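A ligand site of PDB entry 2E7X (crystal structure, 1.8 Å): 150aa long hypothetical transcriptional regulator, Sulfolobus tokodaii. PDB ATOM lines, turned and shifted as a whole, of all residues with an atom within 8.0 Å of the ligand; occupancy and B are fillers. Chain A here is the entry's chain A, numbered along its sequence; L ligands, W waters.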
ATOM      1  N   LEU A  20     -23.816  28.717  12.925  1.00  0.00           N
ATOM      2  CA  LEU A  20     -23.818  27.359  13.462  1.00  0.00           C
ATOM      3  C   LEU A  20     -23.448  26.358  12.376  1.00  0.00           C
ATOM      4  O   LEU A  20     -22.716  25.403  12.637  1.00  0.00           O
ATOM      5  CB  LEU A  20     -25.202  27.015  14.030  1.00  0.00           C
ATOM      6  CG  LEU A  20     -25.584  27.640  15.372  1.00  0.00           C
ATOM      7  CD1 LEU A  20     -27.038  27.318  15.684  1.00  0.00           C
ATOM      8  CD2 LEU A  20     -24.664  27.109  16.464  1.00  0.00           C
ATOM      9  N   ASP A  21     -23.941  26.574  11.162  1.00  0.00           N
ATOM     10  CA  ASP A  21     -23.637  25.666  10.057  1.00  0.00           C
ATOM     11  C   ASP A  21     -22.150  25.628   9.762  1.00  0.00           C
ATOM     12  O   ASP A  21     -21.594  24.561   9.506  1.00  0.00           O
ATOM     13  CB  ASP A  21     -24.394  26.072   8.787  1.00  0.00           C
ATOM     14  CG  ASP A  21     -25.883  25.927   8.920  1.00  0.00           C
ATOM     15  OD1 ASP A  21     -26.329  24.900   9.472  1.00  0.00           O
ATOM     16  OD2 ASP A  21     -26.621  26.823   8.459  1.00  0.00           O
ATOM     17  N   GLU A  22     -21.519  26.794   9.778  1.00  0.00           N
ATOM     18  CA  GLU A  22     -20.088  26.865   9.492  1.00  0.00           C
ATOM     19  C   GLU A  22     -19.274  26.224  10.607  1.00  0.00           C
ATOM     20  O   GLU A  22     -18.306  25.509  10.336  1.00  0.00           O
ATOM     21  CB  GLU A  22     -19.679  28.322   9.279  1.00  0.00           C
ATOM     22  CG  GLU A  22     -20.250  28.894   7.983  1.00  0.00           C
ATOM     23  CD  GLU A  22     -20.023  30.384   7.838  1.00  0.00           C
ATOM     24  OE1 GLU A  22     -20.583  31.152   8.643  1.00  0.00           O
ATOM     25  OE2 GLU A  22     -19.280  30.786   6.918  1.00  0.00           O
ATOM     26  N   ALA A  24     -20.325  23.902  12.774  1.00  0.00           N
ATOM     27  CA  ALA A  24     -20.614  22.473  12.736  1.00  0.00           C
ATOM     28  C   ALA A  24     -19.801  21.792  11.635  1.00  0.00           C
ATOM     29  O   ALA A  24     -19.300  20.681  11.822  1.00  0.00           O
ATOM     30  CB  ALA A  24     -22.104  22.250  12.499  1.00  0.00           C
ATOM     31  N   ARG A  25     -19.673  22.457  10.491  1.00  0.00           N
ATOM     32  CA  ARG A  25     -18.922  21.914   9.365  1.00  0.00           C
ATOM     33  C   ARG A  25     -17.426  21.852   9.699  1.00  0.00           C
ATOM     34  O   ARG A  25     -16.738  20.908   9.322  1.00  0.00           O
ATOM     35  CB  ARG A  25     -19.145  22.780   8.128  1.00  0.00           C
ATOM     36  CG  ARG A  25     -18.427  22.301   6.868  1.00  0.00           C
ATOM     37  CD  ARG A  25     -18.784  23.182   5.679  1.00  0.00           C
ATOM     38  NE  ARG A  25     -20.229  23.345   5.533  1.00  0.00           N
ATOM     39  CZ  ARG A  25     -20.864  24.511   5.571  1.00  0.00           C
ATOM     40  NH1 ARG A  25     -20.183  25.637   5.721  1.00  0.00           N
ATOM     41  NH2 ARG A  25     -22.180  24.550   5.460  1.00  0.00           N
ATOM     42  N   ILE A  29     -19.620  18.157  13.814  1.00  0.00           N
ATOM     43  CA  ILE A  29     -20.610  17.677  14.775  1.00  0.00           C
ATOM     44  C   ILE A  29     -21.969  18.239  14.368  1.00  0.00           C
ATOM     45  O   ILE A  29     -22.040  19.256  13.677  1.00  0.00           O
ATOM     46  CB  ILE A  29     -20.303  18.114  16.239  1.00  0.00           C
ATOM     47  CG1 ILE A  29     -20.377  19.636  16.358  1.00  0.00           C
ATOM     48  CG2 ILE A  29     -18.929  17.613  16.656  1.00  0.00           C
ATOM     49  CD1 ILE A  29     -20.313  20.128  17.797  1.00  0.00           C
ATOM     50  N   PRO A  30     -23.057  17.574  14.776  1.00  0.00           N
ATOM     51  CA  PRO A  30     -24.414  18.023  14.443  1.00  0.00           C
ATOM     52  C   PRO A  30     -24.691  19.433  14.957  1.00  0.00           C
ATOM     53  O   PRO A  30     -24.257  19.791  16.060  1.00  0.00           O
ATOM     54  CB  PRO A  30     -25.301  16.983  15.106  1.00  0.00           C
ATOM     55  CG  PRO A  30     -24.446  15.754  15.105  1.00  0.00           C
ATOM     56  CD  PRO A  30     -23.101  16.295  15.505  1.00  0.00           C
ATOM     57  N   LYS A  31     -25.417  20.217  14.167  1.00  0.00           N
ATOM     58  CA  LYS A  31     -25.753  21.589  14.551  1.00  0.00           C
ATOM     59  C   LYS A  31     -26.574  21.606  15.836  1.00  0.00           C
ATOM     60  O   LYS A  31     -26.421  22.500  16.675  1.00  0.00           O
ATOM     61  CB  LYS A  31     -26.521  22.260  13.417  1.00  0.00           C
ATOM     62  CG  LYS A  31     -26.671  23.760  13.554  1.00  0.00           C
ATOM     63  CD  LYS A  31     -27.168  24.391  12.261  1.00  0.00           C
ATOM     64  CE  LYS A  31     -28.531  23.861  11.869  1.00  0.00           C
ATOM     65  NZ  LYS A  31     -28.583  23.591  10.408  1.00  0.00           N
ATOM     66  N   SER A  32     -27.457  20.624  15.991  1.00  0.00           N
ATOM     67  CA  SER A  32     -28.301  20.541  17.180  1.00  0.00           C
ATOM     68  C   SER A  32     -27.427  20.323  18.423  1.00  0.00           C
ATOM     69  O   SER A  32     -27.670  20.916  19.477  1.00  0.00           O
ATOM     70  CB  SER A  32     -29.312  19.405  17.051  1.00  0.00           C
ATOM     71  OG  SER A  32     -28.663  18.146  17.017  1.00  0.00           O
ATOM     72  N   THR A  33     -26.418  19.466  18.275  1.00  0.00           N
ATOM     73  CA  THR A  33     -25.497  19.164  19.361  1.00  0.00           C
ATOM     74  C   THR A  33     -24.643  20.397  19.659  1.00  0.00           C
ATOM     75  O   THR A  33     -24.331  20.688  20.822  1.00  0.00           O
ATOM     76  CB  THR A  33     -24.572  17.989  18.982  1.00  0.00           C
ATOM     77  OG1 THR A  33     -25.365  16.822  18.729  1.00  0.00           O
ATOM     78  CG2 THR A  33     -23.595  17.684  20.104  1.00  0.00           C
ATOM     79  N   LEU A  34     -24.265  21.120  18.615  1.00  0.00           N
ATOM     80  CA  LEU A  34     -23.471  22.327  18.777  1.00  0.00           C
ATOM     81  C   LEU A  34     -24.246  23.357  19.600  1.00  0.00           C
ATOM     82  O   LEU A  34     -23.717  23.910  20.557  1.00  0.00           O
ATOM     83  CB  LEU A  34     -23.099  22.911  17.417  1.00  0.00           C
ATOM     84  CG  LEU A  34     -22.339  24.232  17.433  1.00  0.00           C
ATOM     85  CD1 LEU A  34     -21.035  24.074  18.206  1.00  0.00           C
ATOM     86  CD2 LEU A  34     -22.059  24.654  15.995  1.00  0.00           C
ATOM     87  N   SER A  35     -25.487  23.611  19.214  1.00  0.00           N
ATOM     88  CA  SER A  35     -26.322  24.577  19.935  1.00  0.00           C
ATOM     89  C   SER A  35     -26.504  24.175  21.390  1.00  0.00           C
ATOM     90  O   SER A  35     -26.496  25.029  22.281  1.00  0.00           O
ATOM     91  CB  SER A  35     -27.686  24.723  19.260  1.00  0.00           C
ATOM     92  OG  SER A  35     -27.577  25.358  18.002  1.00  0.00           O
HETATM   93  N1  LIG L   1     -28.564  16.176  12.186  1.00  0.00           N
HETATM   94  C1  LIG L   1     -28.173  17.606  12.283  1.00  0.00           C
HETATM   95  C2  LIG L   1     -28.670  18.200  13.601  1.00  0.00           C
HETATM   96  O1  LIG L   1     -29.042  17.398  14.480  1.00  0.00           O
HETATM   97  C3  LIG L   1     -28.746  18.391  11.100  1.00  0.00           C
HETATM   98  C4  LIG L   1     -28.217  19.813  10.938  1.00  0.00           C
HETATM   99  C5  LIG L   1     -26.707  19.874  10.781  1.00  0.00           C
HETATM  100  O2  LIG L   1     -26.142  20.941  10.523  1.00  0.00           O
HETATM  101  N2  LIG L   1     -26.037  18.737  10.929  1.00  0.00           N
HETATM  102  O3  LIG L   1     -28.684  19.442  13.733  1.00  0.00           O
HETATM  103  O   HOH W   1     -24.914  15.727  11.266  1.00  0.00           O
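Residues that only touch the ligand: Pro 30 (3.8 Å).
Hydrophobic or aromatic side chains within 4 Å of the ligand: Pro 30.
Three residues have an atom within 4 Å of the ligand: Pro 30, Lys 31 and Ser 32.
The nearest printed residue that does not touch the ligand is Asp 21 (4.1 Å).
N of Ser 32 is in hydrogen-bond range of O3 of the ligand, 2.8 Å away.
The side-chain hydroxyl (OG) of Ser 32 lies within hydrogen-bond range of an oxygen (O1) of the ligand.
An oxygen (O3) of the ligand lies within hydrogen-bond range of the backbone NH (N) of Lys 31, 3.4 Å away.
The side-chain amino group of Lys 31 is in salt-bridge range of the side-chain carboxylate of Asp 21 (2.8 Å).
The side-chain hydroxyl of Ser 35 is in hydrogen-bond range of the backbone carbonyl oxygen of Lys 31 (3.4 Å).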
